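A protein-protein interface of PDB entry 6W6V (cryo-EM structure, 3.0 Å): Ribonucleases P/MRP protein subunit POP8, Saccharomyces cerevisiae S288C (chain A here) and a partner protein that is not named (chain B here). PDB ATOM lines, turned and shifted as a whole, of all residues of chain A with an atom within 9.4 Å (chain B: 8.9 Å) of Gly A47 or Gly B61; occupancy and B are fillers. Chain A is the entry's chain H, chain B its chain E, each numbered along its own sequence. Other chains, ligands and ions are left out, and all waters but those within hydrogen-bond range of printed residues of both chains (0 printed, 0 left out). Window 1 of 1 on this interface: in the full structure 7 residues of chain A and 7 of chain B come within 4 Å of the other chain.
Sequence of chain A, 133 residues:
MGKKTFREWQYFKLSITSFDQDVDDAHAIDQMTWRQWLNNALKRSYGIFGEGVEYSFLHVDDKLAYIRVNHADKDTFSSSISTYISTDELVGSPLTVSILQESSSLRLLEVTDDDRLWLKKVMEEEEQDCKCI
Among the printed residues, pairs that only touch across the chains: Ser A45 with Gly B61, Phe A49 with Asn B59, Gly A47 with Leu B60, Tyr A46 with Tyr B63, Ser A45 with Tyr B63, Ile A48 with Leu B58, Tyr A46 with Gly B61, Ile A48 with Asn B59 and Phe A49 with Leu B60.
The guanidinium group (NE) of Arg A44 lies within salt-bridge range of the side-chain carboxylate (OD2) of Asp B62 (3.7 Å). N of Asp B62 is in hydrogen-bond range of O of Ser A45 (2.9 Å). The backbone NH of Gly B61 lies close to the backbone NH of Gly A47 (2.9 Å).
Of the 17 printed residues of chain A, 6 touch a printed residue of chain B. Printed residues of chain A that touch a printed residue of chain B: Arg A44, Ser A45, Tyr A46, Gly A47, Ile A48 and Phe A49. Of the 17 printed residues of chain B, 6 touch a printed residue of chain A. Printed residues of chain B that touch a printed residue of chain A: Leu B58, Asn B59, Leu B60, Gly B61, Asp B62 and Tyr B63.
O of Ser B55 lies within hydrogen-bond range of ND2 of Asn B59, at 3.3 Å.
Gly A47 touches just these residues of chain B: Leu B60 and Gly B61. Of chain A, only Ser A45, Tyr A46 and Gly A47 come within 4 Å of Gly B61. No residue of chain A comes within 4 Å of Gly B64. Of the printed residues of chain B, Tyr A46 touches Gly B61 (3.6 Å) and Tyr B63 (3.3 Å). Of the printed residues of chain A, Tyr B63 touches Ser A45 and Tyr A46. Printed residues of chain A within 4 Å of Leu B60: Gly A47 and Phe A49. Printed residues of chain B within 4 Å of Ile A48: Leu B58 (3.4 Å) and Asn B59 (3.8 Å). Of the printed residues of chain A, Leu B58 touches Ile A48. Leu B95 touches none of the printed residues of chain A. The nearest printed residue of chain A that does not touch Leu B60 is Tyr A46 (4.3 Å).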
ATOM      1  N   ASN A  39     -23.707  -0.572  -7.380  1.00  0.00           N
ATOM      2  CA  ASN A  39     -22.967  -0.039  -6.242  1.00  0.00           C
ATOM      3  C   ASN A  39     -22.936  -1.036  -5.094  1.00  0.00           C
ATOM      4  O   ASN A  39     -21.898  -1.220  -4.450  1.00  0.00           O
ATOM      5  CB  ASN A  39     -23.579   1.283  -5.789  1.00  0.00           C
ATOM      6  CG  ASN A  39     -23.156   2.440  -6.658  1.00  0.00           C
ATOM      7  OD1 ASN A  39     -22.194   2.337  -7.415  1.00  0.00           O
ATOM      8  ND2 ASN A  39     -23.872   3.551  -6.558  1.00  0.00           N
ATOM      9  N   ASN A  40     -24.063  -1.700  -4.828  1.00  0.00           N
ATOM     10  CA  ASN A  40     -24.078  -2.706  -3.775  1.00  0.00           C
ATOM     11  C   ASN A  40     -23.107  -3.835  -4.084  1.00  0.00           C
ATOM     12  O   ASN A  40     -22.404  -4.321  -3.191  1.00  0.00           O
ATOM     13  CB  ASN A  40     -25.490  -3.251  -3.590  1.00  0.00           C
ATOM     14  CG  ASN A  40     -26.358  -2.332  -2.763  1.00  0.00           C
ATOM     15  OD1 ASN A  40     -25.967  -1.208  -2.455  1.00  0.00           O
ATOM     16  ND2 ASN A  40     -27.541  -2.806  -2.397  1.00  0.00           N
ATOM     17  N   ALA A  41     -23.052  -4.265  -5.347  1.00  0.00           N
ATOM     18  CA  ALA A  41     -22.113  -5.316  -5.728  1.00  0.00           C
ATOM     19  C   ALA A  41     -20.672  -4.865  -5.535  1.00  0.00           C
ATOM     20  O   ALA A  41     -19.866  -5.565  -4.907  1.00  0.00           O
ATOM     21  CB  ALA A  41     -22.352  -5.731  -7.177  1.00  0.00           C
ATOM     22  N   LEU A  42     -20.328  -3.691  -6.064  1.00  0.00           N
ATOM     23  CA  LEU A  42     -18.961  -3.197  -5.973  1.00  0.00           C
ATOM     24  C   LEU A  42     -18.567  -2.794  -4.561  1.00  0.00           C
ATOM     25  O   LEU A  42     -17.384  -2.536  -4.324  1.00  0.00           O
ATOM     26  CB  LEU A  42     -18.768  -2.012  -6.911  1.00  0.00           C
ATOM     27  CG  LEU A  42     -18.744  -2.355  -8.395  1.00  0.00           C
ATOM     28  CD1 LEU A  42     -19.392  -1.247  -9.198  1.00  0.00           C
ATOM     29  CD2 LEU A  42     -17.321  -2.581  -8.848  1.00  0.00           C
ATOM     30  N   LYS A  43     -19.522  -2.705  -3.635  1.00  0.00           N
ATOM     31  CA  LYS A  43     -19.199  -2.488  -2.230  1.00  0.00           C
ATOM     32  C   LYS A  43     -19.046  -3.798  -1.468  1.00  0.00           C
ATOM     33  O   LYS A  43     -18.142  -3.929  -0.638  1.00  0.00           O
ATOM     34  CB  LYS A  43     -20.275  -1.634  -1.563  1.00  0.00           C
ATOM     35  CG  LYS A  43     -20.150  -1.562  -0.058  1.00  0.00           C
ATOM     36  CD  LYS A  43     -21.257  -0.725   0.551  1.00  0.00           C
ATOM     37  CE  LYS A  43     -21.103  -0.634   2.059  1.00  0.00           C
ATOM     38  NZ  LYS A  43     -20.998  -1.981   2.684  1.00  0.00           N
ATOM     39  N   ARG A  44     -19.923  -4.768  -1.722  1.00  0.00           N
ATOM     40  CA  ARG A  44     -19.780  -6.070  -1.082  1.00  0.00           C
ATOM     41  C   ARG A  44     -18.480  -6.738  -1.498  1.00  0.00           C
ATOM     42  O   ARG A  44     -17.781  -7.324  -0.666  1.00  0.00           O
ATOM     43  CB  ARG A  44     -20.973  -6.957  -1.432  1.00  0.00           C
ATOM     44  CG  ARG A  44     -20.940  -8.370  -0.860  1.00  0.00           C
ATOM     45  CD  ARG A  44     -21.157  -8.412   0.651  1.00  0.00           C
ATOM     46  NE  ARG A  44     -19.935  -8.214   1.427  1.00  0.00           N
ATOM     47  CZ  ARG A  44     -19.909  -8.057   2.747  1.00  0.00           C
ATOM     48  NH1 ARG A  44     -21.039  -8.075   3.441  1.00  0.00           N
ATOM     49  NH2 ARG A  44     -18.754  -7.884   3.377  1.00  0.00           N
ATOM     50  N   SER A  45     -18.130  -6.650  -2.780  1.00  0.00           N
ATOM     51  CA  SER A  45     -16.931  -7.319  -3.269  1.00  0.00           C
ATOM     52  C   SER A  45     -15.656  -6.570  -2.900  1.00  0.00           C
ATOM     53  O   SER A  45     -14.755  -7.149  -2.291  1.00  0.00           O
ATOM     54  CB  SER A  45     -17.011  -7.505  -4.784  1.00  0.00           C
ATOM     55  OG  SER A  45     -15.838  -8.126  -5.275  1.00  0.00           O
ATOM     56  N   TYR A  46     -15.552  -5.297  -3.272  1.00  0.00           N
ATOM     57  CA  TYR A  46     -14.420  -4.464  -2.895  1.00  0.00           C
ATOM     58  C   TYR A  46     -14.904  -3.366  -1.961  1.00  0.00           C
ATOM     59  O   TYR A  46     -16.063  -2.954  -2.028  1.00  0.00           O
ATOM     60  CB  TYR A  46     -13.745  -3.837  -4.106  1.00  0.00           C
ATOM     61  CG  TYR A  46     -13.045  -4.822  -5.000  1.00  0.00           C
ATOM     62  CD1 TYR A  46     -12.784  -6.108  -4.576  1.00  0.00           C
ATOM     63  CD2 TYR A  46     -12.615  -4.453  -6.260  1.00  0.00           C
ATOM     64  CE1 TYR A  46     -12.141  -7.004  -5.397  1.00  0.00           C
ATOM     65  CE2 TYR A  46     -11.965  -5.343  -7.082  1.00  0.00           C
ATOM     66  CZ  TYR A  46     -11.731  -6.617  -6.645  1.00  0.00           C
ATOM     67  OH  TYR A  46     -11.083  -7.512  -7.462  1.00  0.00           O
ATOM     68  N   GLY A  47     -14.019  -2.883  -1.102  1.00  0.00           N
ATOM     69  CA  GLY A  47     -14.431  -1.916  -0.105  1.00  0.00           C
ATOM     70  C   GLY A  47     -14.572  -0.506  -0.636  1.00  0.00           C
ATOM     71  O   GLY A  47     -15.049  -0.300  -1.754  1.00  0.00           O
ATOM     72  N   ILE A  48     -14.158   0.474   0.168  1.00  0.00           N
ATOM     73  CA  ILE A  48     -14.240   1.872  -0.239  1.00  0.00           C
ATOM     74  C   ILE A  48     -13.457   2.110  -1.519  1.00  0.00           C
ATOM     75  O   ILE A  48     -13.843   2.941  -2.348  1.00  0.00           O
ATOM     76  CB  ILE A  48     -13.752   2.779   0.907  1.00  0.00           C
ATOM     77  CG1 ILE A  48     -14.641   2.604   2.140  1.00  0.00           C
ATOM     78  CG2 ILE A  48     -13.707   4.231   0.472  1.00  0.00           C
ATOM     79  CD1 ILE A  48     -16.052   3.100   1.950  1.00  0.00           C
ATOM     80  N   PHE A  49     -12.358   1.384  -1.716  1.00  0.00           N
ATOM     81  CA  PHE A  49     -11.611   1.506  -2.959  1.00  0.00           C
ATOM     82  C   PHE A  49     -12.360   0.928  -4.148  1.00  0.00           C
ATOM     83  O   PHE A  49     -11.968   1.187  -5.290  1.00  0.00           O
ATOM     84  CB  PHE A  49     -10.253   0.823  -2.825  1.00  0.00           C
ATOM     85  CG  PHE A  49      -9.186   1.712  -2.265  1.00  0.00           C
ATOM     86  CD1 PHE A  49      -9.285   2.200  -0.975  1.00  0.00           C
ATOM     87  CD2 PHE A  49      -8.090   2.069  -3.027  1.00  0.00           C
ATOM     88  CE1 PHE A  49      -8.311   3.023  -0.455  1.00  0.00           C
ATOM     89  CE2 PHE A  49      -7.111   2.892  -2.511  1.00  0.00           C
ATOM     90  CZ  PHE A  49      -7.223   3.368  -1.223  1.00  0.00           C
ATOM     91  N   GLY A  50     -13.417   0.158  -3.910  1.00  0.00           N
ATOM     92  CA  GLY A  50     -14.214  -0.403  -4.982  1.00  0.00           C
ATOM     93  C   GLY A  50     -15.430   0.435  -5.310  1.00  0.00           C
ATOM     94  O   GLY A  50     -16.388  -0.053  -5.913  1.00  0.00           O
ATOM     95  N   GLU A  51     -15.408   1.699  -4.897  1.00  0.00           N
ATOM     96  CA  GLU A  51     -16.486   2.633  -5.182  1.00  0.00           C
ATOM     97  C   GLU A  51     -16.151   3.593  -6.305  1.00  0.00           C
ATOM     98  O   GLU A  51     -17.061   4.082  -6.981  1.00  0.00           O
ATOM     99  CB  GLU A  51     -16.826   3.447  -3.932  1.00  0.00           C
ATOM    100  CG  GLU A  51     -17.401   2.626  -2.814  1.00  0.00           C
ATOM    101  CD  GLU A  51     -18.751   2.066  -3.162  1.00  0.00           C
ATOM    102  OE1 GLU A  51     -19.490   2.726  -3.920  1.00  0.00           O
ATOM    103  OE2 GLU A  51     -19.071   0.964  -2.682  1.00  0.00           O
ATOM    104  N   GLY A  52     -14.873   3.864  -6.522  1.00  0.00           N
ATOM    105  CA  GLY A  52     -14.446   4.855  -7.480  1.00  0.00           C
ATOM    106  C   GLY A  52     -14.468   4.423  -8.921  1.00  0.00           C
ATOM    107  O   GLY A  52     -14.094   5.213  -9.790  1.00  0.00           O
ATOM    108  N   VAL A  53     -14.881   3.191  -9.211  1.00  0.00           N
ATOM    109  CA  VAL A  53     -15.021   2.760 -10.595  1.00  0.00           C
ATOM    110  C   VAL A  53     -16.072   3.639 -11.260  1.00  0.00           C
ATOM    111  O   VAL A  53     -17.246   3.624 -10.876  1.00  0.00           O
ATOM    112  CB  VAL A  53     -15.380   1.267 -10.691  1.00  0.00           C
ATOM    113  CG1 VAL A  53     -14.173   0.418 -10.371  1.00  0.00           C
ATOM    114  CG2 VAL A  53     -16.497   0.928  -9.734  1.00  0.00           C
ATOM    115  N   THR A  76     -11.737  -5.101 -12.066  1.00  0.00           N
ATOM    116  CA  THR A  76     -12.632  -4.927 -10.929  1.00  0.00           C
ATOM    117  C   THR A  76     -14.067  -5.255 -11.306  1.00  0.00           C
ATOM    118  O   THR A  76     -14.664  -6.197 -10.771  1.00  0.00           O
ATOM    119  CB  THR A  76     -12.529  -3.495 -10.408  1.00  0.00           C
ATOM    120  OG1 THR A  76     -11.209  -3.256  -9.904  1.00  0.00           O
ATOM    121  CG2 THR A  76     -13.548  -3.238  -9.324  1.00  0.00           C
ATOM    122  N   SER A  80     -16.719  -8.479  -9.962  1.00  0.00           N
ATOM    123  CA  SER A  80     -17.701  -8.315  -8.900  1.00  0.00           C
ATOM    124  C   SER A  80     -19.126  -8.548  -9.378  1.00  0.00           C
ATOM    125  O   SER A  80     -19.912  -9.203  -8.684  1.00  0.00           O
ATOM    126  CB  SER A  80     -17.574  -6.922  -8.291  1.00  0.00           C
ATOM    127  OG  SER A  80     -17.462  -5.947  -9.308  1.00  0.00           O
ATOM    128  N   ARG B  53      -6.219  -6.098  10.662  1.00  0.00           N
ATOM    129  CA  ARG B  53      -7.293  -6.833  10.005  1.00  0.00           C
ATOM    130  C   ARG B  53      -8.554  -5.987   9.888  1.00  0.00           C
ATOM    131  O   ARG B  53      -9.287  -6.102   8.902  1.00  0.00           O
ATOM    132  CB  ARG B  53      -7.592  -8.129  10.752  1.00  0.00           C
ATOM    133  CG  ARG B  53      -6.669  -9.277  10.400  1.00  0.00           C
ATOM    134  CD  ARG B  53      -6.625 -10.288  11.526  1.00  0.00           C
ATOM    135  NE  ARG B  53      -6.509 -11.656  11.038  1.00  0.00           N
ATOM    136  CZ  ARG B  53      -6.454 -12.723  11.827  1.00  0.00           C
ATOM    137  NH1 ARG B  53      -6.505 -12.577  13.143  1.00  0.00           N
ATOM    138  NH2 ARG B  53      -6.350 -13.935  11.300  1.00  0.00           N
ATOM    139  N   SER B  55      -8.660  -2.732   9.417  1.00  0.00           N
ATOM    140  CA  SER B  55      -8.457  -1.697   8.412  1.00  0.00           C
ATOM    141  C   SER B  55      -8.457  -2.229   6.990  1.00  0.00           C
ATOM    142  O   SER B  55      -8.432  -1.427   6.053  1.00  0.00           O
ATOM    143  CB  SER B  55      -7.141  -0.964   8.663  1.00  0.00           C
ATOM    144  OG  SER B  55      -6.711  -0.303   7.488  1.00  0.00           O
ATOM    145  N   LEU B  56      -8.466  -3.544   6.799  1.00  0.00           N
ATOM    146  CA  LEU B  56      -8.486  -4.124   5.463  1.00  0.00           C
ATOM    147  C   LEU B  56      -9.888  -4.461   4.985  1.00  0.00           C
ATOM    148  O   LEU B  56     -10.229  -4.170   3.838  1.00  0.00           O
ATOM    149  CB  LEU B  56      -7.619  -5.384   5.414  1.00  0.00           C
ATOM    150  CG  LEU B  56      -6.140  -5.157   5.102  1.00  0.00           C
ATOM    151  CD1 LEU B  56      -5.365  -6.453   5.207  1.00  0.00           C
ATOM    152  CD2 LEU B  56      -5.971  -4.535   3.729  1.00  0.00           C
ATOM    153  N   SER B  57     -10.716  -5.053   5.839  1.00  0.00           N
ATOM    154  CA  SER B  57     -12.073  -5.417   5.459  1.00  0.00           C
ATOM    155  C   SER B  57     -13.023  -4.230   5.448  1.00  0.00           C
ATOM    156  O   SER B  57     -14.238  -4.431   5.357  1.00  0.00           O
ATOM    157  CB  SER B  57     -12.611  -6.497   6.399  1.00  0.00           C
ATOM    158  OG  SER B  57     -12.791  -5.983   7.705  1.00  0.00           O
ATOM    159  N   LEU B  58     -12.506  -3.013   5.549  1.00  0.00           N
ATOM    160  CA  LEU B  58     -13.303  -1.798   5.437  1.00  0.00           C
ATOM    161  C   LEU B  58     -12.829  -0.891   4.318  1.00  0.00           C
ATOM    162  O   LEU B  58     -13.653  -0.313   3.608  1.00  0.00           O
ATOM    163  CB  LEU B  58     -13.283  -1.028   6.765  1.00  0.00           C
ATOM    164  CG  LEU B  58     -14.287   0.108   6.966  1.00  0.00           C
ATOM    165  CD1 LEU B  58     -14.630   0.223   8.438  1.00  0.00           C
ATOM    166  CD2 LEU B  58     -13.750   1.432   6.452  1.00  0.00           C
ATOM    167  N   ASN B  59     -11.521  -0.740   4.150  1.00  0.00           N
ATOM    168  CA  ASN B  59     -10.969   0.005   3.033  1.00  0.00           C
ATOM    169  C   ASN B  59     -10.762  -0.866   1.806  1.00  0.00           C
ATOM    170  O   ASN B  59     -10.442  -0.341   0.737  1.00  0.00           O
ATOM    171  CB  ASN B  59      -9.644   0.646   3.439  1.00  0.00           C
ATOM    172  CG  ASN B  59      -9.827   1.766   4.435  1.00  0.00           C
ATOM    173  OD1 ASN B  59     -10.740   2.577   4.314  1.00  0.00           O
ATOM    174  ND2 ASN B  59      -8.968   1.803   5.442  1.00  0.00           N
ATOM    175  N   LEU B  60     -10.925  -2.177   1.948  1.00  0.00           N
ATOM    176  CA  LEU B  60     -10.923  -3.119   0.841  1.00  0.00           C
ATOM    177  C   LEU B  60     -11.982  -4.168   1.141  1.00  0.00           C
ATOM    178  O   LEU B  60     -12.479  -4.269   2.265  1.00  0.00           O
ATOM    179  CB  LEU B  60      -9.546  -3.755   0.637  1.00  0.00           C
ATOM    180  CG  LEU B  60      -8.420  -2.801   0.237  1.00  0.00           C
ATOM    181  CD1 LEU B  60      -7.068  -3.441   0.445  1.00  0.00           C
ATOM    182  CD2 LEU B  60      -8.580  -2.366  -1.202  1.00  0.00           C
ATOM    183  N   GLY B  61     -12.344  -4.944   0.136  1.00  0.00           N
ATOM    184  CA  GLY B  61     -13.460  -5.852   0.259  1.00  0.00           C
ATOM    185  C   GLY B  61     -13.046  -7.261   0.624  1.00  0.00           C
ATOM    186  O   GLY B  61     -11.986  -7.492   1.214  1.00  0.00           O
ATOM    187  N   ASP B  62     -13.908  -8.218   0.279  1.00  0.00           N
ATOM    188  CA  ASP B  62     -13.591  -9.620   0.519  1.00  0.00           C
ATOM    189  C   ASP B  62     -12.396 -10.067  -0.309  1.00  0.00           C
ATOM    190  O   ASP B  62     -11.517 -10.774   0.193  1.00  0.00           O
ATOM    191  CB  ASP B  62     -14.807 -10.486   0.216  1.00  0.00           C
ATOM    192  CG  ASP B  62     -15.922 -10.275   1.207  1.00  0.00           C
ATOM    193  OD1 ASP B  62     -15.622  -9.937   2.369  1.00  0.00           O
ATOM    194  OD2 ASP B  62     -17.098 -10.446   0.830  1.00  0.00           O
ATOM    195  N   TYR B  63     -12.340  -9.661  -1.574  1.00  0.00           N
ATOM    196  CA  TYR B  63     -11.232 -10.032  -2.441  1.00  0.00           C
ATOM    197  C   TYR B  63      -9.995  -9.187  -2.203  1.00  0.00           C
ATOM    198  O   TYR B  63      -9.004  -9.351  -2.919  1.00  0.00           O
ATOM    199  CB  TYR B  63     -11.643  -9.926  -3.908  1.00  0.00           C
ATOM    200  CG  TYR B  63     -12.569 -11.014  -4.384  1.00  0.00           C
ATOM    201  CD1 TYR B  63     -12.258 -12.349  -4.198  1.00  0.00           C
ATOM    202  CD2 TYR B  63     -13.750 -10.703  -5.035  1.00  0.00           C
ATOM    203  CE1 TYR B  63     -13.101 -13.341  -4.638  1.00  0.00           C
ATOM    204  CE2 TYR B  63     -14.597 -11.687  -5.478  1.00  0.00           C
ATOM    205  CZ  TYR B  63     -14.269 -13.003  -5.278  1.00  0.00           C
ATOM    206  OH  TYR B  63     -15.117 -13.985  -5.722  1.00  0.00           O
ATOM    207  N   GLY B  64     -10.033  -8.278  -1.237  1.00  0.00           N
ATOM    208  CA  GLY B  64      -8.849  -7.537  -0.859  1.00  0.00           C
ATOM    209  C   GLY B  64      -8.370  -7.944   0.517  1.00  0.00           C
ATOM    210  O   GLY B  64      -7.187  -7.808   0.841  1.00  0.00           O
ATOM    211  N   SER B  65      -9.291  -8.448   1.335  1.00  0.00           N
ATOM    212  CA  SER B  65      -8.980  -8.934   2.670  1.00  0.00           C
ATOM    213  C   SER B  65      -8.736 -10.431   2.714  1.00  0.00           C
ATOM    214  O   SER B  65      -8.488 -10.969   3.795  1.00  0.00           O
ATOM    215  CB  SER B  65     -10.107  -8.578   3.639  1.00  0.00           C
ATOM    216  OG  SER B  65     -10.003  -9.348   4.821  1.00  0.00           O
ATOM    217  N   ALA B  66      -8.817 -11.118   1.577  1.00  0.00           N
ATOM    218  CA  ALA B  66      -8.523 -12.539   1.517  1.00  0.00           C
ATOM    219  C   ALA B  66      -7.248 -12.859   0.758  1.00  0.00           C
ATOM    220  O   ALA B  66      -6.681 -13.934   0.965  1.00  0.00           O
ATOM    221  CB  ALA B  66      -9.686 -13.304   0.874  1.00  0.00           C
ATOM    222  N   LYS B  67      -6.787 -11.962  -0.107  1.00  0.00           N
ATOM    223  CA  LYS B  67      -5.518 -12.155  -0.789  1.00  0.00           C
ATOM    224  C   LYS B  67      -4.323 -11.821   0.090  1.00  0.00           C
ATOM    225  O   LYS B  67      -3.191 -12.134  -0.289  1.00  0.00           O
ATOM    226  CB  LYS B  67      -5.474 -11.311  -2.064  1.00  0.00           C
ATOM    227  CG  LYS B  67      -5.926 -12.054  -3.305  1.00  0.00           C
ATOM    228  CD  LYS B  67      -6.597 -11.125  -4.297  1.00  0.00           C
ATOM    229  CE  LYS B  67      -5.613 -10.125  -4.866  1.00  0.00           C
ATOM    230  NZ  LYS B  67      -6.299  -9.096  -5.693  1.00  0.00           N
ATOM    231  N   CYS B  68      -4.544 -11.197   1.244  1.00  0.00           N
ATOM    232  CA  CYS B  68      -3.484 -10.881   2.194  1.00  0.00           C
ATOM    233  C   CYS B  68      -3.548 -11.721   3.455  1.00  0.00           C
ATOM    234  O   CYS B  68      -2.508 -12.065   4.015  1.00  0.00           O
ATOM    235  CB  CYS B  68      -3.544  -9.402   2.582  1.00  0.00           C
ATOM    236  SG  CYS B  68      -3.362  -8.274   1.195  1.00  0.00           S
ATOM    237  N   ASN B  69      -4.751 -12.067   3.909  1.00  0.00           N
ATOM    238  CA  ASN B  69      -4.925 -12.846   5.126  1.00  0.00           C
ATOM    239  C   ASN B  69      -4.487 -14.294   4.969  1.00  0.00           C
ATOM    240  O   ASN B  69      -4.448 -15.020   5.967  1.00  0.00           O
ATOM    241  CB  ASN B  69      -6.386 -12.791   5.569  1.00  0.00           C
ATOM    242  CG  ASN B  69      -6.560 -13.083   7.041  1.00  0.00           C
ATOM    243  OD1 ASN B  69      -5.586 -13.186   7.785  1.00  0.00           O
ATOM    244  ND2 ASN B  69      -7.808 -13.216   7.471  1.00  0.00           N
ATOM    245  N   LEU B  95      -1.117  -3.954  -0.506  1.00  0.00           N
ATOM    246  CA  LEU B  95      -2.379  -3.867   0.216  1.00  0.00           C
ATOM    247  C   LEU B  95      -2.150  -3.777   1.721  1.00  0.00           C
ATOM    248  O   LEU B  95      -2.881  -3.071   2.426  1.00  0.00           O
ATOM    249  CB  LEU B  95      -3.257  -5.064  -0.134  1.00  0.00           C
ATOM    250  CG  LEU B  95      -3.351  -5.419  -1.620  1.00  0.00           C
ATOM    251  CD1 LEU B  95      -4.387  -6.508  -1.837  1.00  0.00           C
ATOM    252  CD2 LEU B  95      -3.678  -4.194  -2.461  1.00  0.00           C
